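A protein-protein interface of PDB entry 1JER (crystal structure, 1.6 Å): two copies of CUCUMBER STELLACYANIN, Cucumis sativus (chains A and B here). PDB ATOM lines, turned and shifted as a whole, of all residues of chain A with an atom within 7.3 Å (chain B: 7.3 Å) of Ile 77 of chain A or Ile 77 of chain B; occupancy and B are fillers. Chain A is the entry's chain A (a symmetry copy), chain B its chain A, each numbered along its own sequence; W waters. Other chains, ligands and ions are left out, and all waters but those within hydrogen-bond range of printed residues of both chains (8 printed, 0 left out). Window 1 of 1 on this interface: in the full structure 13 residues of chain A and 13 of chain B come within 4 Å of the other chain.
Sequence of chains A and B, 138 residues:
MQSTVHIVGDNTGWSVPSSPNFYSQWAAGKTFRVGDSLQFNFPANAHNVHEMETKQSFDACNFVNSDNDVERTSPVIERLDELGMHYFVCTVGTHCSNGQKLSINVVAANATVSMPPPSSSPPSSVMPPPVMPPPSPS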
ATOM      1  N   THR A   4      25.518  14.677  -6.568  1.00  0.00           N
ATOM      2  CA  THR A   4      25.381  13.543  -7.510  1.00  0.00           C
ATOM      3  C   THR A   4      23.905  13.301  -7.792  1.00  0.00           C
ATOM      4  O   THR A   4      23.088  13.332  -6.887  1.00  0.00           O
ATOM      5  CB  THR A   4      25.926  12.273  -6.758  1.00  0.00           C
ATOM      6  OG1 THR A   4      27.349  12.526  -6.587  1.00  0.00           O
ATOM      7  CG2 THR A   4      25.875  11.050  -7.644  1.00  0.00           C
ATOM      8  N   VAL A   5      23.618  12.890  -9.033  1.00  0.00           N
ATOM      9  CA  VAL A   5      22.205  12.418  -9.281  1.00  0.00           C
ATOM     10  C   VAL A   5      22.331  10.899  -9.382  1.00  0.00           C
ATOM     11  O   VAL A   5      23.017  10.345 -10.260  1.00  0.00           O
ATOM     12  CB  VAL A   5      21.704  12.998 -10.614  1.00  0.00           C
ATOM     13  CG1 VAL A   5      20.270  12.470 -10.887  1.00  0.00           C
ATOM     14  CG2 VAL A   5      21.688  14.529 -10.551  1.00  0.00           C
ATOM     15  N   HIS A   6      21.791  10.195  -8.395  1.00  0.00           N
ATOM     16  CA  HIS A   6      22.005   8.721  -8.414  1.00  0.00           C
ATOM     17  C   HIS A   6      20.848   8.107  -9.247  1.00  0.00           C
ATOM     18  O   HIS A   6      19.715   8.546  -9.074  1.00  0.00           O
ATOM     19  CB  HIS A   6      21.864   8.203  -6.989  1.00  0.00           C
ATOM     20  CG  HIS A   6      22.818   8.843  -6.031  1.00  0.00           C
ATOM     21  ND1 HIS A   6      24.089   8.307  -5.825  1.00  0.00           N
ATOM     22  CD2 HIS A   6      22.653   9.907  -5.204  1.00  0.00           C
ATOM     23  CE1 HIS A   6      24.689   9.061  -4.887  1.00  0.00           C
ATOM     24  NE2 HIS A   6      23.860  10.026  -4.509  1.00  0.00           N
ATOM     25  N   ILE A   7      21.166   7.123 -10.032  1.00  0.00           N
ATOM     26  CA  ILE A   7      20.104   6.466 -10.842  1.00  0.00           C
ATOM     27  C   ILE A   7      19.677   5.200 -10.086  1.00  0.00           C
ATOM     28  O   ILE A   7      20.446   4.294  -9.905  1.00  0.00           O
ATOM     29  CB  ILE A   7      20.689   6.045 -12.211  1.00  0.00           C
ATOM     30  CG1 ILE A   7      21.218   7.274 -13.007  1.00  0.00           C
ATOM     31  CG2 ILE A   7      19.531   5.420 -13.036  1.00  0.00           C
ATOM     32  CD1 ILE A   7      20.126   8.324 -13.198  1.00  0.00           C
ATOM     33  N   ASP A  36      22.139  15.759  -2.990  1.00  0.00           N
ATOM     34  CA  ASP A  36      22.127  14.815  -4.155  1.00  0.00           C
ATOM     35  C   ASP A  36      20.622  14.615  -4.509  1.00  0.00           C
ATOM     36  O   ASP A  36      19.749  14.963  -3.771  1.00  0.00           O
ATOM     37  CB  ASP A  36      22.561  13.414  -3.584  1.00  0.00           C
ATOM     38  CG  ASP A  36      24.058  13.340  -3.415  1.00  0.00           C
ATOM     39  OD1 ASP A  36      24.756  14.317  -3.749  1.00  0.00           O
ATOM     40  OD2 ASP A  36      24.557  12.299  -2.919  1.00  0.00           O
ATOM     41  N   SER A  37      20.460  13.945  -5.677  1.00  0.00           N
ATOM     42  CA  SER A  37      19.053  13.645  -6.058  1.00  0.00           C
ATOM     43  C   SER A  37      19.005  12.144  -6.437  1.00  0.00           C
ATOM     44  O   SER A  37      20.021  11.531  -6.696  1.00  0.00           O
ATOM     45  CB  SER A  37      18.775  14.455  -7.379  1.00  0.00           C
ATOM     46  OG  SER A  37      18.702  15.848  -7.056  1.00  0.00           O
ATOM     47  N   LEU A  38      17.769  11.640  -6.471  1.00  0.00           N
ATOM     48  CA  LEU A  38      17.565  10.211  -6.828  1.00  0.00           C
ATOM     49  C   LEU A  38      16.653  10.279  -8.118  1.00  0.00           C
ATOM     50  O   LEU A  38      15.653  10.953  -8.039  1.00  0.00           O
ATOM     51  CB  LEU A  38      16.633   9.588  -5.777  1.00  0.00           C
ATOM     52  CG  LEU A  38      17.214   9.198  -4.445  1.00  0.00           C
ATOM     53  CD1 LEU A  38      16.204   8.393  -3.637  1.00  0.00           C
ATOM     54  CD2 LEU A  38      18.519   8.410  -4.641  1.00  0.00           C
ATOM     55  N   GLN A  39      17.126   9.610  -9.138  1.00  0.00           N
ATOM     56  CA  GLN A  39      16.326   9.576 -10.380  1.00  0.00           C
ATOM     57  C   GLN A  39      15.693   8.171 -10.525  1.00  0.00           C
ATOM     58  O   GLN A  39      16.455   7.199 -10.582  1.00  0.00           O
ATOM     59  CB  GLN A  39      17.211   9.840 -11.593  1.00  0.00           C
ATOM     60  CG  GLN A  39      16.409   9.696 -12.897  1.00  0.00           C
ATOM     61  CD  GLN A  39      17.100  10.367 -14.057  1.00  0.00           C
ATOM     62  OE1 GLN A  39      17.880  11.305 -13.853  1.00  0.00           O
ATOM     63  NE2 GLN A  39      16.815   9.900 -15.264  1.00  0.00           N
ATOM     64  N   PHE A  40      14.378   8.134 -10.621  1.00  0.00           N
ATOM     65  CA  PHE A  40      13.679   6.811 -10.792  1.00  0.00           C
ATOM     66  C   PHE A  40      13.172   6.790 -12.277  1.00  0.00           C
ATOM     67  O   PHE A  40      12.437   7.691 -12.632  1.00  0.00           O
ATOM     68  CB  PHE A  40      12.401   6.891  -9.923  1.00  0.00           C
ATOM     69  CG  PHE A  40      12.705   6.801  -8.423  1.00  0.00           C
ATOM     70  CD1 PHE A  40      13.026   7.975  -7.732  1.00  0.00           C
ATOM     71  CD2 PHE A  40      12.628   5.622  -7.739  1.00  0.00           C
ATOM     72  CE1 PHE A  40      13.224   7.909  -6.344  1.00  0.00           C
ATOM     73  CE2 PHE A  40      12.861   5.543  -6.361  1.00  0.00           C
ATOM     74  CZ  PHE A  40      13.197   6.717  -5.686  1.00  0.00           C
ATOM     75  N   ASN A  41      13.655   5.815 -13.016  1.00  0.00           N
ATOM     76  CA  ASN A  41      13.288   5.679 -14.444  1.00  0.00           C
ATOM     77  C   ASN A  41      12.410   4.405 -14.572  1.00  0.00           C
ATOM     78  O   ASN A  41      12.772   3.333 -14.098  1.00  0.00           O
ATOM     79  CB  ASN A  41      14.579   5.367 -15.255  1.00  0.00           C
ATOM     80  CG  ASN A  41      15.493   6.596 -15.325  1.00  0.00           C
ATOM     81  OD1 ASN A  41      15.082   7.713 -15.397  1.00  0.00           O
ATOM     82  ND2 ASN A  41      16.810   6.269 -15.350  1.00  0.00           N
ATOM     83  N   VAL A  49       6.251   6.737  -7.699  1.00  0.00           N
ATOM     84  CA  VAL A  49       7.228   6.901  -6.622  1.00  0.00           C
ATOM     85  C   VAL A  49       6.572   7.750  -5.522  1.00  0.00           C
ATOM     86  O   VAL A  49       6.109   8.841  -5.799  1.00  0.00           O
ATOM     87  CB  VAL A  49       8.467   7.692  -7.111  1.00  0.00           C
ATOM     88  CG1 VAL A  49       9.439   7.759  -5.891  1.00  0.00           C
ATOM     89  CG2 VAL A  49       9.153   6.930  -8.244  1.00  0.00           C
ATOM     90  N   THR A  73       4.352   9.744 -14.430  1.00  0.00           N
ATOM     91  CA  THR A  73       5.291  10.075 -15.507  1.00  0.00           C
ATOM     92  C   THR A  73       6.725   9.806 -14.977  1.00  0.00           C
ATOM     93  O   THR A  73       6.967   9.886 -13.789  1.00  0.00           O
ATOM     94  CB  THR A  73       5.217  11.581 -15.843  1.00  0.00           C
ATOM     95  OG1 THR A  73       5.317  12.315 -14.610  1.00  0.00           O
ATOM     96  CG2 THR A  73       3.824  11.871 -16.416  1.00  0.00           C
ATOM     97  N   SER A  74       7.584   9.473 -15.889  1.00  0.00           N
ATOM     98  CA  SER A  74       8.985   9.134 -15.575  1.00  0.00           C
ATOM     99  C   SER A  74       9.838  10.008 -16.500  1.00  0.00           C
ATOM    100  O   SER A  74       9.356  10.282 -17.615  1.00  0.00           O
ATOM    101  CB  SER A  74       9.206   7.653 -15.865  1.00  0.00           C
ATOM    102  OG  SER A  74      10.617   7.302 -15.878  1.00  0.00           O
ATOM    103  N   PRO A  75      11.001  10.403 -16.089  1.00  0.00           N
ATOM    104  CA  PRO A  75      11.600  10.059 -14.808  1.00  0.00           C
ATOM    105  C   PRO A  75      11.104  10.960 -13.677  1.00  0.00           C
ATOM    106  O   PRO A  75      10.689  12.101 -13.940  1.00  0.00           O
ATOM    107  CB  PRO A  75      13.104  10.461 -15.040  1.00  0.00           C
ATOM    108  CG  PRO A  75      12.984  11.620 -15.975  1.00  0.00           C
ATOM    109  CD  PRO A  75      11.883  11.223 -16.953  1.00  0.00           C
ATOM    110  N   VAL A  76      11.152  10.408 -12.476  1.00  0.00           N
ATOM    111  CA  VAL A  76      10.810  11.172 -11.257  1.00  0.00           C
ATOM    112  C   VAL A  76      12.155  11.439 -10.553  1.00  0.00           C
ATOM    113  O   VAL A  76      12.927  10.474 -10.410  1.00  0.00           O
ATOM    114  CB  VAL A  76       9.960  10.338 -10.306  1.00  0.00           C
ATOM    115  CG1 VAL A  76       9.916  11.032  -8.921  1.00  0.00           C
ATOM    116  CG2 VAL A  76       8.530  10.252 -10.878  1.00  0.00           C
ATOM    117  N   ILE A  77      12.446  12.692 -10.300  1.00  0.00           N
ATOM    118  CA  ILE A  77      13.810  12.963  -9.675  1.00  0.00           C
ATOM    119  C   ILE A  77      13.538  13.618  -8.333  1.00  0.00           C
ATOM    120  O   ILE A  77      12.832  14.632  -8.260  1.00  0.00           O
ATOM    121  CB  ILE A  77      14.625  13.904 -10.594  1.00  0.00           C
ATOM    122  CG1 ILE A  77      15.056  13.167 -11.906  1.00  0.00           C
ATOM    123  CG2 ILE A  77      15.968  14.244  -9.861  1.00  0.00           C
ATOM    124  CD1 ILE A  77      14.939  14.011 -13.137  1.00  0.00           C
ATOM    125  N   GLU A  78      13.985  12.979  -7.249  1.00  0.00           N
ATOM    126  CA  GLU A  78      13.669  13.506  -5.908  1.00  0.00           C
ATOM    127  C   GLU A  78      14.959  14.077  -5.296  1.00  0.00           C
ATOM    128  O   GLU A  78      15.974  13.423  -5.359  1.00  0.00           O
ATOM    129  CB  GLU A  78      13.227  12.303  -5.009  1.00  0.00           C
ATOM    130  CG  GLU A  78      11.846  11.770  -5.491  1.00  0.00           C
ATOM    131  CD  GLU A  78      10.713  12.622  -4.954  1.00  0.00           C
ATOM    132  OE1 GLU A  78      10.909  13.316  -3.930  1.00  0.00           O
ATOM    133  OE2 GLU A  78       9.591  12.564  -5.519  1.00  0.00           O
ATOM    134  N   ARG A  79      14.843  15.268  -4.725  1.00  0.00           N
ATOM    135  CA  ARG A  79      16.002  15.894  -4.097  1.00  0.00           C
ATOM    136  C   ARG A  79      16.135  15.394  -2.662  1.00  0.00           C
ATOM    137  O   ARG A  79      15.154  15.261  -1.947  1.00  0.00           O
ATOM    138  CB  ARG A  79      15.901  17.441  -4.068  1.00  0.00           C
ATOM    139  CG  ARG A  79      17.323  18.051  -3.946  1.00  0.00           C
ATOM    140  CD  ARG A  79      17.344  19.558  -4.171  1.00  0.00           C
ATOM    141  NE  ARG A  79      18.501  19.948  -5.027  1.00  0.00           N
ATOM    142  CZ  ARG A  79      19.662  20.353  -4.543  1.00  0.00           C
ATOM    143  NH1 ARG A  79      19.705  20.946  -3.349  1.00  0.00           N
ATOM    144  NH2 ARG A  79      20.807  20.202  -5.232  1.00  0.00           N
ATOM    145  N   THR B   4      10.718  14.718 -20.455  1.00  0.00           N
ATOM    146  CA  THR B   4      12.065  15.219 -20.806  1.00  0.00           C
ATOM    147  C   THR B   4      12.672  15.915 -19.595  1.00  0.00           C
ATOM    148  O   THR B   4      11.998  16.664 -18.909  1.00  0.00           O
ATOM    149  CB  THR B   4      11.858  16.313 -21.917  1.00  0.00           C
ATOM    150  OG1 THR B   4      11.353  15.580 -23.069  1.00  0.00           O
ATOM    151  CG2 THR B   4      13.180  16.871 -22.388  1.00  0.00           C
ATOM    152  N   VAL B   5      13.998  15.784 -19.464  1.00  0.00           N
ATOM    153  CA  VAL B   5      14.664  16.647 -18.418  1.00  0.00           C
ATOM    154  C   VAL B   5      15.389  17.720 -19.226  1.00  0.00           C
ATOM    155  O   VAL B   5      16.289  17.445 -20.040  1.00  0.00           O
ATOM    156  CB  VAL B   5      15.677  15.798 -17.632  1.00  0.00           C
ATOM    157  CG1 VAL B   5      16.393  16.702 -16.592  1.00  0.00           C
ATOM    158  CG2 VAL B   5      14.960  14.651 -16.912  1.00  0.00           C
ATOM    159  N   HIS B   6      14.913  18.955 -19.128  1.00  0.00           N
ATOM    160  CA  HIS B   6      15.532  19.994 -19.999  1.00  0.00           C
ATOM    161  C   HIS B   6      16.734  20.584 -19.212  1.00  0.00           C
ATOM    162  O   HIS B   6      16.585  20.816 -18.017  1.00  0.00           O
ATOM    163  CB  HIS B   6      14.520  21.115 -20.192  1.00  0.00           C
ATOM    164  CG  HIS B   6      13.232  20.650 -20.793  1.00  0.00           C
ATOM    165  ND1 HIS B   6      13.065  20.608 -22.179  1.00  0.00           N
ATOM    166  CD2 HIS B   6      12.067  20.280 -20.202  1.00  0.00           C
ATOM    167  CE1 HIS B   6      11.806  20.199 -22.412  1.00  0.00           C
ATOM    168  NE2 HIS B   6      11.195  19.986 -21.253  1.00  0.00           N
ATOM    169  N   ILE B   7      17.800  20.845 -19.905  1.00  0.00           N
ATOM    170  CA  ILE B   7      18.984  21.438 -19.226  1.00  0.00           C
ATOM    171  C   ILE B   7      18.936  22.953 -19.476  1.00  0.00           C
ATOM    172  O   ILE B   7      19.038  23.403 -20.584  1.00  0.00           O
ATOM    173  CB  ILE B   7      20.277  20.878 -19.861  1.00  0.00           C
ATOM    174  CG1 ILE B   7      20.359  19.329 -19.717  1.00  0.00           C
ATOM    175  CG2 ILE B   7      21.476  21.481 -19.080  1.00  0.00           C
ATOM    176  CD1 ILE B   7      20.259  18.903 -18.254  1.00  0.00           C
ATOM    177  N   ASP B  36       7.660  17.001 -17.163  1.00  0.00           N
ATOM    178  CA  ASP B  36       9.102  17.198 -17.524  1.00  0.00           C
ATOM    179  C   ASP B  36       9.759  17.840 -16.265  1.00  0.00           C
ATOM    180  O   ASP B  36       9.105  18.291 -15.373  1.00  0.00           O
ATOM    181  CB  ASP B  36       9.130  18.357 -18.588  1.00  0.00           C
ATOM    182  CG  ASP B  36       8.756  17.844 -19.956  1.00  0.00           C
ATOM    183  OD1 ASP B  36       8.509  16.631 -20.104  1.00  0.00           O
ATOM    184  OD2 ASP B  36       8.683  18.662 -20.907  1.00  0.00           O
ATOM    185  N   SER B  37      11.111  17.889 -16.367  1.00  0.00           N
ATOM    186  CA  SER B  37      11.819  18.555 -15.240  1.00  0.00           C
ATOM    187  C   SER B  37      12.813  19.560 -15.870  1.00  0.00           C
ATOM    188  O   SER B  37      13.134  19.475 -17.039  1.00  0.00           O
ATOM    189  CB  SER B  37      12.684  17.437 -14.546  1.00  0.00           C
ATOM    190  OG  SER B  37      11.807  16.542 -13.855  1.00  0.00           O
ATOM    191  N   LEU B  38      13.273  20.470 -15.008  1.00  0.00           N
ATOM    192  CA  LEU B  38      14.243  21.499 -15.469  1.00  0.00           C
ATOM    193  C   LEU B  38      15.511  21.245 -14.559  1.00  0.00           C
ATOM    194  O   LEU B  38      15.320  21.193 -13.367  1.00  0.00           O
ATOM    195  CB  LEU B  38      13.742  22.871 -14.990  1.00  0.00           C
ATOM    196  CG  LEU B  38      12.634  23.537 -15.760  1.00  0.00           C
ATOM    197  CD1 LEU B  38      12.439  24.972 -15.283  1.00  0.00           C
ATOM    198  CD2 LEU B  38      12.926  23.490 -17.268  1.00  0.00           C
ATOM    199  N   GLN B  39      16.623  21.086 -15.230  1.00  0.00           N
ATOM    200  CA  GLN B  39      17.873  20.884 -14.469  1.00  0.00           C
ATOM    201  C   GLN B  39      18.718  22.178 -14.550  1.00  0.00           C
ATOM    202  O   GLN B  39      19.060  22.573 -15.671  1.00  0.00           O
ATOM    203  CB  GLN B  39      18.680  19.736 -15.063  1.00  0.00           C
ATOM    204  CG  GLN B  39      20.034  19.591 -14.347  1.00  0.00           C
ATOM    205  CD  GLN B  39      20.651  18.236 -14.584  1.00  0.00           C
ATOM    206  OE1 GLN B  39      19.931  17.266 -14.851  1.00  0.00           O
ATOM    207  NE2 GLN B  39      21.970  18.162 -14.480  1.00  0.00           N
ATOM    208  N   PHE B  40      19.044  22.731 -13.399  1.00  0.00           N
ATOM    209  CA  PHE B  40      19.889  23.978 -13.383  1.00  0.00           C
ATOM    210  C   PHE B  40      21.298  23.529 -12.861  1.00  0.00           C
ATOM    211  O   PHE B  40      21.348  22.986 -11.775  1.00  0.00           O
ATOM    212  CB  PHE B  40      19.303  24.873 -12.264  1.00  0.00           C
ATOM    213  CG  PHE B  40      17.964  25.505 -12.657  1.00  0.00           C
ATOM    214  CD1 PHE B  40      16.788  24.777 -12.436  1.00  0.00           C
ATOM    215  CD2 PHE B  40      17.882  26.766 -13.173  1.00  0.00           C
ATOM    216  CE1 PHE B  40      15.555  25.384 -12.720  1.00  0.00           C
ATOM    217  CE2 PHE B  40      16.657  27.364 -13.492  1.00  0.00           C
ATOM    218  CZ  PHE B  40      15.494  26.623 -13.283  1.00  0.00           C
ATOM    219  N   ASN B  41      22.293  23.731 -13.698  1.00  0.00           N
ATOM    220  CA  ASN B  41      23.677  23.335 -13.358  1.00  0.00           C
ATOM    221  C   ASN B  41      24.493  24.641 -13.163  1.00  0.00           C
ATOM    222  O   ASN B  41      24.477  25.533 -14.006  1.00  0.00           O
ATOM    223  CB  ASN B  41      24.309  22.641 -14.599  1.00  0.00           C
ATOM    224  CG  ASN B  41      23.682  21.262 -14.836  1.00  0.00           C
ATOM    225  OD1 ASN B  41      23.332  20.543 -13.951  1.00  0.00           O
ATOM    226  ND2 ASN B  41      23.621  20.933 -16.151  1.00  0.00           N
ATOM    227  N   VAL B  49      18.454  28.686  -7.017  1.00  0.00           N
ATOM    228  CA  VAL B  49      17.263  28.633  -7.865  1.00  0.00           C
ATOM    229  C   VAL B  49      16.034  28.770  -6.953  1.00  0.00           C
ATOM    230  O   VAL B  49      15.885  28.000  -6.023  1.00  0.00           O
ATOM    231  CB  VAL B  49      17.141  27.259  -8.568  1.00  0.00           C
ATOM    232  CG1 VAL B  49      15.866  27.350  -9.465  1.00  0.00           C
ATOM    233  CG2 VAL B  49      18.357  27.026  -9.464  1.00  0.00           C
ATOM    234  N   THR B  73      23.432  24.070  -3.571  1.00  0.00           N
ATOM    235  CA  THR B  73      24.081  22.909  -4.190  1.00  0.00           C
ATOM    236  C   THR B  73      23.483  22.741  -5.612  1.00  0.00           C
ATOM    237  O   THR B  73      22.355  23.123  -5.855  1.00  0.00           O
ATOM    238  CB  THR B  73      23.739  21.620  -3.409  1.00  0.00           C
ATOM    239  OG1 THR B  73      22.312  21.579  -3.225  1.00  0.00           O
ATOM    240  CG2 THR B  73      24.357  21.734  -2.010  1.00  0.00           C
ATOM    241  N   SER B  74      24.287  22.204  -6.476  1.00  0.00           N
ATOM    242  CA  SER B  74      23.917  22.003  -7.889  1.00  0.00           C
ATOM    243  C   SER B  74      24.210  20.530  -8.188  1.00  0.00           C
ATOM    244  O   SER B  74      25.161  20.012  -7.573  1.00  0.00           O
ATOM    245  CB  SER B  74      24.778  22.919  -8.755  1.00  0.00           C
ATOM    246  OG  SER B  74      24.700  22.574 -10.164  1.00  0.00           O
ATOM    247  N   PRO B  75      23.477  19.911  -9.057  1.00  0.00           N
ATOM    248  CA  PRO B  75      22.390  20.510  -9.818  1.00  0.00           C
ATOM    249  C   PRO B  75      21.084  20.552  -9.025  1.00  0.00           C
ATOM    250  O   PRO B  75      20.892  19.727  -8.116  1.00  0.00           O
ATOM    251  CB  PRO B  75      22.164  19.440 -10.951  1.00  0.00           C
ATOM    252  CG  PRO B  75      22.509  18.163 -10.256  1.00  0.00           C
ATOM    253  CD  PRO B  75      23.735  18.495  -9.410  1.00  0.00           C
ATOM    254  N   VAL B  76      20.252  21.513  -9.389  1.00  0.00           N
ATOM    255  CA  VAL B  76      18.901  21.634  -8.801  1.00  0.00           C
ATOM    256  C   VAL B  76      17.932  21.171  -9.907  1.00  0.00           C
ATOM    257  O   VAL B  76      18.092  21.649 -11.044  1.00  0.00           O
ATOM    258  CB  VAL B  76      18.566  23.088  -8.488  1.00  0.00           C
ATOM    259  CG1 VAL B  76      17.047  23.211  -8.205  1.00  0.00           C
ATOM    260  CG2 VAL B  76      19.354  23.509  -7.230  1.00  0.00           C
ATOM    261  N   ILE B  77      17.116  20.192  -9.599  1.00  0.00           N
ATOM    262  CA  ILE B  77      16.212  19.681 -10.715  1.00  0.00           C
ATOM    263  C   ILE B  77      14.787  19.913 -10.247  1.00  0.00           C
ATOM    264  O   ILE B  77      14.404  19.468  -9.156  1.00  0.00           O
ATOM    265  CB  ILE B  77      16.478  18.174 -10.950  1.00  0.00           C
ATOM    266  CG1 ILE B  77      17.884  17.951 -11.599  1.00  0.00           C
ATOM    267  CG2 ILE B  77      15.452  17.669 -12.023  1.00  0.00           C
ATOM    268  CD1 ILE B  77      18.628  16.779 -11.037  1.00  0.00           C
ATOM    269  N   GLU B  78      14.028  20.714 -10.997  1.00  0.00           N
ATOM    270  CA  GLU B  78      12.667  21.065 -10.548  1.00  0.00           C
ATOM    271  C   GLU B  78      11.657  20.347 -11.460  1.00  0.00           C
ATOM    272  O   GLU B  78      11.823  20.384 -12.657  1.00  0.00           O
ATOM    273  CB  GLU B  78      12.469  22.601 -10.764  1.00  0.00           C
ATOM    274  CG  GLU B  78      13.362  23.390  -9.761  1.00  0.00           C
ATOM    275  CD  GLU B  78      12.712  23.471  -8.394  1.00  0.00           C
ATOM    276  OE1 GLU B  78      11.471  23.323  -8.304  1.00  0.00           O
ATOM    277  OE2 GLU B  78      13.429  23.740  -7.397  1.00  0.00           O
ATOM    278  N   ARG B  79      10.656  19.740 -10.838  1.00  0.00           N
ATOM    279  CA  ARG B  79       9.631  19.044 -11.609  1.00  0.00           C
ATOM    280  C   ARG B  79       8.555  20.037 -12.038  1.00  0.00           C
ATOM    281  O   ARG B  79       8.148  20.895 -11.270  1.00  0.00           O
ATOM    282  CB  ARG B  79       8.952  17.904 -10.805  1.00  0.00           C
ATOM    283  CG  ARG B  79       8.337  16.873 -11.788  1.00  0.00           C
ATOM    284  CD  ARG B  79       7.879  15.594 -11.097  1.00  0.00           C
ATOM    285  NE  ARG B  79       8.269  14.396 -11.893  1.00  0.00           N
ATOM    286  CZ  ARG B  79       7.467  13.803 -12.760  1.00  0.00           C
ATOM    287  NH1 ARG B  79       6.146  13.878 -12.590  1.00  0.00           N
ATOM    288  NH2 ARG B  79       7.946  13.105 -13.804  1.00  0.00           N
HETATM  289  O   HOH W   1       5.255  10.603 -11.901  1.00  0.00           O
HETATM  290  O   HOH W   2      10.902  14.860 -11.515  1.00  0.00           O
HETATM  291  O   HOH W   3       3.331  14.409 -13.796  1.00  0.00           O
HETATM  292  O   HOH W   4      20.991  16.987  -7.046  1.00  0.00           O
HETATM  293  O   HOH W   5      20.667  24.184  -4.113  1.00  0.00           O
HETATM  294  O   HOH W   6      10.913  14.673 -15.353  1.00  0.00           O
HETATM  295  O   HOH W   7      17.515  18.623  -7.163  1.00  0.00           O
HETATM  296  O   HOH W   8      21.024  21.197  -0.545  1.00  0.00           O
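Asp 36 of chain A touches none of the printed residues of chain B.
Of chain B, only Val 5 (3.8 Å) and Ile 77 (3.9 Å) come within 4 Å of Ile 77 of chain A.
Of the printed residues of chain A, Val 5 of chain B touches Pro 75 (3.7 Å) and Ile 77 (3.8 Å).
Printed residues of chain A within 4 Å of Thr 73 of chain B: Arg 79 (2.7 Å).
Printed residues of chain A within 4 Å of Pro 75 of chain B: Val 5 (3.7 Å) and Arg 79 (2.9 Å).
Of the printed residues of chain A, Arg 79 of chain B touches Thr 73 and Pro 75.
The nearest residue of chain A that does not touch Ile 77 of chain B is Ser 37 of chain A (4.1 Å).
Val 5 of chain A touches Ile 77 of chain B, and with the chains exchanged Ile 77 of chain A touches Val 5 of chain B.
Thr 73 of chain A touches Arg 79 of chain B, and with the chains exchanged Arg 79 of chain A touches Thr 73 of chain B.
Pro 75 of chain A touches Arg 79 of chain B, and with the chains exchanged Arg 79 of chain A touches Pro 75 of chain B.
Ile 77 of chain B touches its own counterpart, Ile 77 of chain A.
18 positions are printed for both chains.
Of the 9 pairs that touch across the chains among the printed residues, 9 have their exchanged pair printed and touching as well.
Among the printed residues, pairs that only touch across the chains: Val 5 of chain A with Pro 75 of chain B (3.7 Å), Pro 75 of chain A with Val 5 of chain B (3.7 Å), Ile 77 of chain A with Val 5 of chain B (3.8 Å), Val 5 of chain A with Ile 77 of chain B (3.8 Å) and Ile 77 of chain A with Ile 77 of chain B (3.9 Å).
Of the 18 printed residues of chain B, 5 touch a printed residue of chain A.
Hydrophobic or aromatic side chains of chain A within 4 Å of the printed part of chain B: Val 5, Pro 75 and Ile 77.
Among the printed residues, 9 pairs touch across the chains.
Among the printed residues, no Asp or Glu carboxylate lies within 4 Å of a Lys or Arg side-chain nitrogen of the other chain.
The guanidinium group (NH1) of Arg 79 of chain A lies within hydrogen-bond range of the side-chain hydroxyl (OG1) of Thr 73 of chain B (2.7 Å).
The backbone carbonyl oxygen (O) of Pro 75 of chain B lies within hydrogen-bond range of the guanidinium group (NH2) of Arg 79 of chain A (2.9 Å).
The side-chain hydroxyl (OG1) of Thr 73 of chain A is in hydrogen-bond range of the guanidinium group (NH1) of Arg 79 of chain B (2.7 Å).
The guanidinium group (NH2) of Arg 79 of chain B lies within hydrogen-bond range of the backbone carbonyl oxygen (O) of Pro 75 of chain A, 2.9 Å away.
Water W4 lies within hydrogen-bond range of the side-chain hydroxyl of Ser 37 of chain A and the backbone carbonyl oxygen of Pro 75 of chain B.
Water W6 lies within hydrogen-bond range of the side-chain hydroxyl (OG) of Ser 37 of chain B (2.6 Å) and the backbone carbonyl oxygen (O) of Pro 75 of chain A (2.9 Å).
Water W1 lies within hydrogen-bond range of the backbone carbonyl oxygen of Thr 73 of chain A and the guanidinium group of Arg 79 of chain B.
Water W5 lies within hydrogen-bond range of O of Thr 73 of chain B (2.6 Å) and NH1 of Arg 79 of chain A (3.5 Å).
Water W7 lies within hydrogen-bond range of the guanidinium group of Arg 79 of chain A (2.7 Å), the backbone NH of Ile 77 of chain B (2.9 Å) and the side-chain hydroxyl of Ser 37 of chain A (3.0 Å).
Water W3 bridges the side-chain hydroxyl (OG1) of Thr 73 of chain A (3.0 Å) and the guanidinium group (NH1) of Arg 79 of chain B (3.1 Å).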
